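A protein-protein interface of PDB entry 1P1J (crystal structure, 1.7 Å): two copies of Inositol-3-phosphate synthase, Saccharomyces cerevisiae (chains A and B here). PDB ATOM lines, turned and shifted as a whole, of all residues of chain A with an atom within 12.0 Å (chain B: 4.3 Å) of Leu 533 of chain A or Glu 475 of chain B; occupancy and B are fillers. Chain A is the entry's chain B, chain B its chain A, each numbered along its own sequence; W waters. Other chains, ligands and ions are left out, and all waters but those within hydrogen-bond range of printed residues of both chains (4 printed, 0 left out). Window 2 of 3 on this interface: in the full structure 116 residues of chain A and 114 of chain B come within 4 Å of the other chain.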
ATOM      1  N   GLU A 122     -24.110  -7.731  15.140  1.00  0.00           N
ATOM      2  CA  GLU A 122     -24.704  -7.671  13.805  1.00  0.00           C
ATOM      3  C   GLU A 122     -24.510  -6.293  13.176  1.00  0.00           C
ATOM      4  O   GLU A 122     -24.788  -6.094  11.992  1.00  0.00           O
ATOM      5  CB  GLU A 122     -26.201  -7.988  13.876  1.00  0.00           C
ATOM      6  CG  GLU A 122     -26.644  -8.676  15.164  1.00  0.00           C
ATOM      7  CD  GLU A 122     -25.981 -10.022  15.382  1.00  0.00           C
ATOM      8  OE1 GLU A 122     -26.221 -10.634  16.444  1.00  0.00           O
ATOM      9  OE2 GLU A 122     -25.225 -10.471  14.496  1.00  0.00           O
ATOM     10  N   GLY A 123     -24.037  -5.344  13.977  1.00  0.00           N
ATOM     11  CA  GLY A 123     -23.815  -3.996  13.482  1.00  0.00           C
ATOM     12  C   GLY A 123     -25.019  -3.091  13.666  1.00  0.00           C
ATOM     13  O   GLY A 123     -25.080  -2.003  13.088  1.00  0.00           O
ATOM     14  N   LEU A 526     -21.772   7.890  11.509  1.00  0.00           N
ATOM     15  CA  LEU A 526     -21.052   7.532  10.290  1.00  0.00           C
ATOM     16  C   LEU A 526     -21.258   6.073   9.885  1.00  0.00           C
ATOM     17  O   LEU A 526     -21.207   5.742   8.701  1.00  0.00           O
ATOM     18  CB  LEU A 526     -19.560   7.847  10.444  1.00  0.00           C
ATOM     19  CG  LEU A 526     -19.226   9.346  10.486  1.00  0.00           C
ATOM     20  CD1 LEU A 526     -17.770   9.535  10.862  1.00  0.00           C
ATOM     21  CD2 LEU A 526     -19.519   9.989   9.131  1.00  0.00           C
ATOM     22  N   ARG A 527     -21.484   5.204  10.866  1.00  0.00           N
ATOM     23  CA  ARG A 527     -21.739   3.788  10.607  1.00  0.00           C
ATOM     24  C   ARG A 527     -20.834   3.173   9.535  1.00  0.00           C
ATOM     25  O   ARG A 527     -21.315   2.531   8.596  1.00  0.00           O
ATOM     26  CB  ARG A 527     -23.206   3.617  10.206  1.00  0.00           C
ATOM     27  CG  ARG A 527     -24.163   4.187  11.238  1.00  0.00           C
ATOM     28  CD  ARG A 527     -25.611   4.198  10.764  1.00  0.00           C
ATOM     29  NE  ARG A 527     -26.497   4.552  11.872  1.00  0.00           N
ATOM     30  CZ  ARG A 527     -26.886   3.699  12.815  1.00  0.00           C
ATOM     31  NH1 ARG A 527     -26.480   2.437  12.781  1.00  0.00           N
ATOM     32  NH2 ARG A 527     -27.664   4.112  13.805  1.00  0.00           N
ATOM     33  N   PHE A 528     -19.526   3.347   9.690  1.00  0.00           N
ATOM     34  CA  PHE A 528     -18.583   2.814   8.718  1.00  0.00           C
ATOM     35  C   PHE A 528     -18.588   1.294   8.632  1.00  0.00           C
ATOM     36  O   PHE A 528     -18.143   0.724   7.634  1.00  0.00           O
ATOM     37  CB  PHE A 528     -17.175   3.341   9.011  1.00  0.00           C
ATOM     38  CG  PHE A 528     -16.955   4.759   8.551  1.00  0.00           C
ATOM     39  CD1 PHE A 528     -15.813   5.459   8.922  1.00  0.00           C
ATOM     40  CD2 PHE A 528     -17.880   5.386   7.714  1.00  0.00           C
ATOM     41  CE1 PHE A 528     -15.590   6.755   8.469  1.00  0.00           C
ATOM     42  CE2 PHE A 528     -17.667   6.684   7.256  1.00  0.00           C
ATOM     43  CZ  PHE A 528     -16.517   7.370   7.634  1.00  0.00           C
ATOM     44  N   GLU A 529     -19.103   0.635   9.667  1.00  0.00           N
ATOM     45  CA  GLU A 529     -19.179  -0.822   9.655  1.00  0.00           C
ATOM     46  C   GLU A 529     -20.076  -1.266   8.498  1.00  0.00           C
ATOM     47  O   GLU A 529     -19.879  -2.335   7.918  1.00  0.00           O
ATOM     48  CB  GLU A 529     -19.746  -1.356  10.976  1.00  0.00           C
ATOM     49  CG  GLU A 529     -18.815  -1.227  12.176  1.00  0.00           C
ATOM     50  CD  GLU A 529     -18.800   0.165  12.787  1.00  0.00           C
ATOM     51  OE1 GLU A 529     -18.031   0.377  13.750  1.00  0.00           O
ATOM     52  OE2 GLU A 529     -19.556   1.043  12.322  1.00  0.00           O
ATOM     53  N   GLU A 530     -21.066  -0.439   8.170  1.00  0.00           N
ATOM     54  CA  GLU A 530     -21.987  -0.746   7.081  1.00  0.00           C
ATOM     55  C   GLU A 530     -21.655  -0.036   5.770  1.00  0.00           C
ATOM     56  O   GLU A 530     -21.718  -0.639   4.698  1.00  0.00           O
ATOM     57  CB  GLU A 530     -23.430  -0.396   7.476  1.00  0.00           C
ATOM     58  CG  GLU A 530     -24.385  -0.349   6.283  1.00  0.00           C
ATOM     59  CD  GLU A 530     -25.848  -0.218   6.669  1.00  0.00           C
ATOM     60  OE1 GLU A 530     -26.157   0.496   7.647  1.00  0.00           O
ATOM     61  OE2 GLU A 530     -26.695  -0.822   5.978  1.00  0.00           O
ATOM     62  N   ARG A 531     -21.297   1.241   5.855  1.00  0.00           N
ATOM     63  CA  ARG A 531     -21.019   2.026   4.658  1.00  0.00           C
ATOM     64  C   ARG A 531     -19.716   1.701   3.928  1.00  0.00           C
ATOM     65  O   ARG A 531     -19.634   1.863   2.710  1.00  0.00           O
ATOM     66  CB  ARG A 531     -21.071   3.521   4.995  1.00  0.00           C
ATOM     67  CG  ARG A 531     -22.389   3.965   5.656  1.00  0.00           C
ATOM     68  CD  ARG A 531     -22.456   5.485   5.776  1.00  0.00           C
ATOM     69  NE  ARG A 531     -23.179   5.940   6.966  1.00  0.00           N
ATOM     70  CZ  ARG A 531     -24.477   6.226   7.016  1.00  0.00           C
ATOM     71  NH1 ARG A 531     -25.243   6.110   5.938  1.00  0.00           N
ATOM     72  NH2 ARG A 531     -25.008   6.648   8.155  1.00  0.00           N
ATOM     73  N   LEU A 532     -18.703   1.249   4.661  1.00  0.00           N
ATOM     74  CA  LEU A 532     -17.423   0.918   4.042  1.00  0.00           C
ATOM     75  C   LEU A 532     -17.298  -0.594   3.886  1.00  0.00           C
ATOM     76  O   LEU A 532     -17.936  -1.357   4.611  1.00  0.00           O
ATOM     77  CB  LEU A 532     -16.269   1.465   4.890  1.00  0.00           C
ATOM     78  CG  LEU A 532     -16.390   2.938   5.298  1.00  0.00           C
ATOM     79  CD1 LEU A 532     -15.144   3.362   6.062  1.00  0.00           C
ATOM     80  CD2 LEU A 532     -16.577   3.810   4.061  1.00  0.00           C
ATOM     81  N   LEU A 533     -16.485  -1.025   2.928  1.00  0.00           N
ATOM     82  CA  LEU A 533     -16.298  -2.448   2.682  1.00  0.00           C
ATOM     83  C   LEU A 533     -15.811  -3.180   3.924  1.00  0.00           C
ATOM     84  O   LEU A 533     -16.434  -4.205   4.278  1.00  0.00           O
ATOM     85  CB  LEU A 533     -15.316  -2.659   1.527  1.00  0.00           C
ATOM     86  CG  LEU A 533     -15.823  -2.229   0.146  1.00  0.00           C
ATOM     87  CD1 LEU A 533     -14.742  -2.462  -0.900  1.00  0.00           C
ATOM     88  CD2 LEU A 533     -17.074  -3.014  -0.202  1.00  0.00           C
ATOM     89  OXT LEU A 533     -14.813  -2.724   4.524  1.00  0.00           O
ATOM     90  N   SER B 460     -12.772   7.608  -2.148  1.00  0.00           N
ATOM     91  CA  SER B 460     -12.222   6.274  -1.936  1.00  0.00           C
ATOM     92  C   SER B 460     -11.524   6.317  -0.577  1.00  0.00           C
ATOM     93  O   SER B 460     -11.372   7.389   0.012  1.00  0.00           O
ATOM     94  CB  SER B 460     -11.244   5.872  -3.057  1.00  0.00           C
ATOM     95  OG  SER B 460     -10.200   6.810  -3.229  1.00  0.00           O
ATOM     96  N   TYR B 461     -11.105   5.162  -0.073  1.00  0.00           N
ATOM     97  CA  TYR B 461     -10.467   5.118   1.239  1.00  0.00           C
ATOM     98  C   TYR B 461      -9.755   3.791   1.453  1.00  0.00           C
ATOM     99  O   TYR B 461      -9.973   2.828   0.721  1.00  0.00           O
ATOM    100  CB  TYR B 461     -11.536   5.273   2.317  1.00  0.00           C
ATOM    101  CG  TYR B 461     -12.599   4.211   2.179  1.00  0.00           C
ATOM    102  CD1 TYR B 461     -12.433   2.950   2.755  1.00  0.00           C
ATOM    103  CD2 TYR B 461     -13.713   4.421   1.364  1.00  0.00           C
ATOM    104  CE1 TYR B 461     -13.341   1.923   2.517  1.00  0.00           C
ATOM    105  CE2 TYR B 461     -14.623   3.403   1.117  1.00  0.00           C
ATOM    106  CZ  TYR B 461     -14.431   2.155   1.692  1.00  0.00           C
ATOM    107  OH  TYR B 461     -15.321   1.141   1.424  1.00  0.00           O
ATOM    108  N   LYS B 463      -8.017   1.351   4.922  1.00  0.00           N
ATOM    109  CA  LYS B 463      -7.776   1.229   6.351  1.00  0.00           C
ATOM    110  C   LYS B 463      -6.296   1.486   6.579  1.00  0.00           C
ATOM    111  O   LYS B 463      -5.465   1.121   5.747  1.00  0.00           O
ATOM    112  CB  LYS B 463      -8.119  -0.176   6.848  1.00  0.00           C
ATOM    113  CG  LYS B 463      -9.574  -0.582   6.700  1.00  0.00           C
ATOM    114  CD  LYS B 463      -9.817  -1.923   7.383  1.00  0.00           C
ATOM    115  CE  LYS B 463     -11.240  -2.416   7.183  1.00  0.00           C
ATOM    116  NZ  LYS B 463     -11.528  -2.720   5.754  1.00  0.00           N
ATOM    117  N   LYS B 473      -4.824  -0.984  -0.070  1.00  0.00           N
ATOM    118  CA  LYS B 473      -5.133  -0.079  -1.171  1.00  0.00           C
ATOM    119  C   LYS B 473      -6.521   0.544  -1.047  1.00  0.00           C
ATOM    120  O   LYS B 473      -7.366   0.070  -0.285  1.00  0.00           O
ATOM    121  CB  LYS B 473      -4.993  -0.812  -2.513  1.00  0.00           C
ATOM    122  CG  LYS B 473      -5.733  -2.140  -2.614  1.00  0.00           C
ATOM    123  CD  LYS B 473      -7.229  -1.957  -2.808  1.00  0.00           C
ATOM    124  CE  LYS B 473      -7.921  -3.298  -3.004  1.00  0.00           C
ATOM    125  NZ  LYS B 473      -9.381  -3.143  -3.247  1.00  0.00           N
ATOM    126  N   PHE B 474      -6.745   1.614  -1.800  1.00  0.00           N
ATOM    127  CA  PHE B 474      -8.021   2.314  -1.764  1.00  0.00           C
ATOM    128  C   PHE B 474      -9.175   1.532  -2.367  1.00  0.00           C
ATOM    129  O   PHE B 474      -9.018   0.839  -3.374  1.00  0.00           O
ATOM    130  CB  PHE B 474      -7.902   3.665  -2.467  1.00  0.00           C
ATOM    131  CG  PHE B 474      -7.038   4.646  -1.740  1.00  0.00           C
ATOM    132  CD1 PHE B 474      -5.667   4.693  -1.973  1.00  0.00           C
ATOM    133  CD2 PHE B 474      -7.589   5.508  -0.798  1.00  0.00           C
ATOM    134  CE1 PHE B 474      -4.859   5.588  -1.276  1.00  0.00           C
ATOM    135  CE2 PHE B 474      -6.792   6.403  -0.096  1.00  0.00           C
ATOM    136  CZ  PHE B 474      -5.425   6.446  -0.334  1.00  0.00           C
ATOM    137  N   GLU B 475     -10.341   1.659  -1.738  1.00  0.00           N
ATOM    138  CA  GLU B 475     -11.552   0.989  -2.186  1.00  0.00           C
ATOM    139  C   GLU B 475     -12.681   2.013  -2.200  1.00  0.00           C
ATOM    140  O   GLU B 475     -12.570   3.069  -1.582  1.00  0.00           O
ATOM    141  CB  GLU B 475     -11.921  -0.145  -1.229  1.00  0.00           C
ATOM    142  CG  GLU B 475     -10.850  -1.202  -1.063  1.00  0.00           C
ATOM    143  CD  GLU B 475     -11.279  -2.308  -0.120  1.00  0.00           C
ATOM    144  OE1 GLU B 475     -11.536  -2.014   1.068  1.00  0.00           O
ATOM    145  OE2 GLU B 475     -11.362  -3.471  -0.568  1.00  0.00           O
ATOM    146  N   ASN B 476     -13.762   1.704  -2.906  1.00  0.00           N
ATOM    147  CA  ASN B 476     -14.901   2.614  -2.959  1.00  0.00           C
ATOM    148  C   ASN B 476     -15.909   2.197  -1.895  1.00  0.00           C
ATOM    149  O   ASN B 476     -15.738   1.170  -1.241  1.00  0.00           O
ATOM    150  CB  ASN B 476     -15.557   2.571  -4.342  1.00  0.00           C
ATOM    151  CG  ASN B 476     -14.592   2.929  -5.453  1.00  0.00           C
ATOM    152  OD1 ASN B 476     -13.918   3.957  -5.397  1.00  0.00           O
ATOM    153  ND2 ASN B 476     -14.524   2.083  -6.473  1.00  0.00           N
ATOM    154  N   TYR B 478     -19.180   0.718   0.011  1.00  0.00           N
ATOM    155  CA  TYR B 478     -19.898  -0.525  -0.201  1.00  0.00           C
ATOM    156  C   TYR B 478     -21.029  -0.045  -1.126  1.00  0.00           C
ATOM    157  O   TYR B 478     -21.636   0.999  -0.877  1.00  0.00           O
ATOM    158  CB  TYR B 478     -20.450  -1.067   1.123  1.00  0.00           C
ATOM    159  CG  TYR B 478     -21.477  -2.155   0.941  1.00  0.00           C
ATOM    160  CD1 TYR B 478     -22.842  -1.860   0.975  1.00  0.00           C
ATOM    161  CD2 TYR B 478     -21.093  -3.473   0.687  1.00  0.00           C
ATOM    162  CE1 TYR B 478     -23.796  -2.846   0.757  1.00  0.00           C
ATOM    163  CE2 TYR B 478     -22.045  -4.471   0.465  1.00  0.00           C
ATOM    164  CZ  TYR B 478     -23.393  -4.147   0.502  1.00  0.00           C
ATOM    165  OH  TYR B 478     -24.343  -5.111   0.274  1.00  0.00           O
ATOM    166  N   ARG B 494     -27.361  -2.999   3.714  1.00  0.00           N
ATOM    167  CA  ARG B 494     -26.411  -4.075   3.505  1.00  0.00           C
ATOM    168  C   ARG B 494     -27.014  -5.253   4.258  1.00  0.00           C
ATOM    169  O   ARG B 494     -27.562  -5.080   5.348  1.00  0.00           O
ATOM    170  CB  ARG B 494     -25.064  -3.677   4.108  1.00  0.00           C
ATOM    171  CG  ARG B 494     -23.934  -4.670   3.916  1.00  0.00           C
ATOM    172  CD  ARG B 494     -22.631  -3.991   4.269  1.00  0.00           C
ATOM    173  NE  ARG B 494     -21.460  -4.831   4.053  1.00  0.00           N
ATOM    174  CZ  ARG B 494     -20.211  -4.394   4.168  1.00  0.00           C
ATOM    175  NH1 ARG B 494     -19.981  -3.130   4.495  1.00  0.00           N
ATOM    176  NH2 ARG B 494     -19.191  -5.217   3.962  1.00  0.00           N
HETATM  177  O   HOH W   1     -13.527  -4.516   6.384  1.00  0.00           O
HETATM  178  O   HOH W   2     -13.100  -0.967   4.408  1.00  0.00           O
HETATM  179  O   HOH W   3     -13.679  -0.495   6.971  1.00  0.00           O
HETATM  180  O   HOH W   4     -22.032   2.829   1.422  1.00  0.00           O
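The side-chain hydroxyl (OH) of Tyr 461 of chain B is in hydrogen-bond range of the backbone NH (N) of Leu 533 of chain A, 2.9 Å away.
The chain-end carboxylate (OXT) of Leu 533 of chain A lies within salt-bridge range of the side-chain amino group (NZ) of Lys 463 of chain B (3.5 Å).
O of Arg 531 of chain A sits at hydrogen-bond distance from N of Tyr 478 of chain B.
The guanidinium group of Arg 494 of chain B sits at hydrogen-bond distance from the backbone carbonyl oxygen of Glu 530 of chain A, at 3.0 Å.
The backbone carbonyl oxygen (O) of Leu 532 of chain A sits at hydrogen-bond distance from the guanidinium group (NH1) of Arg 494 of chain B (2.7 Å).
The guanidinium group (NH2) of Arg 494 of chain B is in salt-bridge range of the chain-end carboxylate (O) of Leu 533 of chain A, at 3.0 Å.
The backbone NH (N) of Glu 475 of chain B sits at hydrogen-bond distance from the backbone carbonyl oxygen (O) of Tyr 461 of chain B, at 2.7 Å.
The side-chain hydroxyl (OH) of Tyr 461 of chain B is in hydrogen-bond range of the backbone carbonyl oxygen (O) of Asn 476 of chain B (2.7 Å).
NZ of Lys 473 of chain B is in salt-bridge range of OE2 of Glu 475 of chain B (3.3 Å).
The backbone carbonyl oxygen of Leu 526 of chain A lies within hydrogen-bond range of the guanidinium group of Arg 531 of chain A.
Among the printed residues, merely in contact across the chains: Leu 532 of chain A with Tyr 461 of chain B (3.4 Å), Glu 529 of chain A with Arg 494 of chain B (3.5 Å), Leu 533 of chain A with Glu 475 of chain B (3.5 Å), Leu 533 of chain A with Asn 476 of chain B (3.7 Å), Leu 533 of chain A with Tyr 478 of chain B (3.8 Å) and Glu 530 of chain A with Tyr 478 of chain B (3.8 Å).
Leu 533 of chain A touches six residues of chain B.
Of chain A, only Leu 533 comes within 4 Å of Glu 475 of chain B.
Of chain A, only Leu 532 and Leu 533 come within 4 Å of Tyr 461 of chain B.
No residue of chain A comes within 4 Å of Lys 473 of chain B.
Phe 474 of chain B touches none of the printed residues of chain A.
Of chain A, only Leu 533 (3.7 Å) comes within 4 Å of Asn 476 of chain B.
Of chain A, only Glu 530 (3.8 Å), Arg 531 (3.0 Å) and Leu 533 (3.8 Å) come within 4 Å of Tyr 478 of chain B.
Printed residues of chain B within 4 Å of Arg 531 of chain A: Tyr 478 (3.0 Å).
Printed residues of chain B within 4 Å of Glu 530 of chain A: Tyr 478 and Arg 494.
Gly 123 of chain A touches none of the printed residues of chain B.
Phe 528 of chain A touches none of the printed residues of chain B.
The nearest printed residue of chain B that does not touch Leu 533 of chain A is Lys 473 of chain B (5.9 Å).
The nearest residue of chain A that does not touch Glu 475 of chain B is Leu 532 of chain A (6.6 Å).
The nearest printed residue of chain B that does not touch Glu 530 of chain A is Tyr 461 of chain B (7.4 Å).
Along chain B the printed residues that touch a printed residue of chain A span positions 461 to 494.
Hydrophobic or aromatic side chains of chain A that line the printed part of chain B: Leu 532 and Leu 533.
Among the printed residues, 12 pairs touch across the chains.
No position is printed for both chains.
Water W2 lies within hydrogen-bond range of OXT of Leu 533 of chain A and NZ of Lys 463 of chain B.
Water W1 lies within hydrogen-bond range of NZ of Lys 463 of chain B (2.8 Å) and OXT of Leu 533 of chain A (2.9 Å).
Water W4 lies within hydrogen-bond range of the backbone carbonyl oxygen of Arg 531 of chain A (2.9 Å) and the backbone carbonyl oxygen of Tyr 478 of chain B (3.0 Å).
Water W3 bridges the side-chain amino group (NZ) of Lys 463 of chain B (3.3 Å) and the chain-end carboxylate (OXT) of Leu 533 of chain A (3.5 Å).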
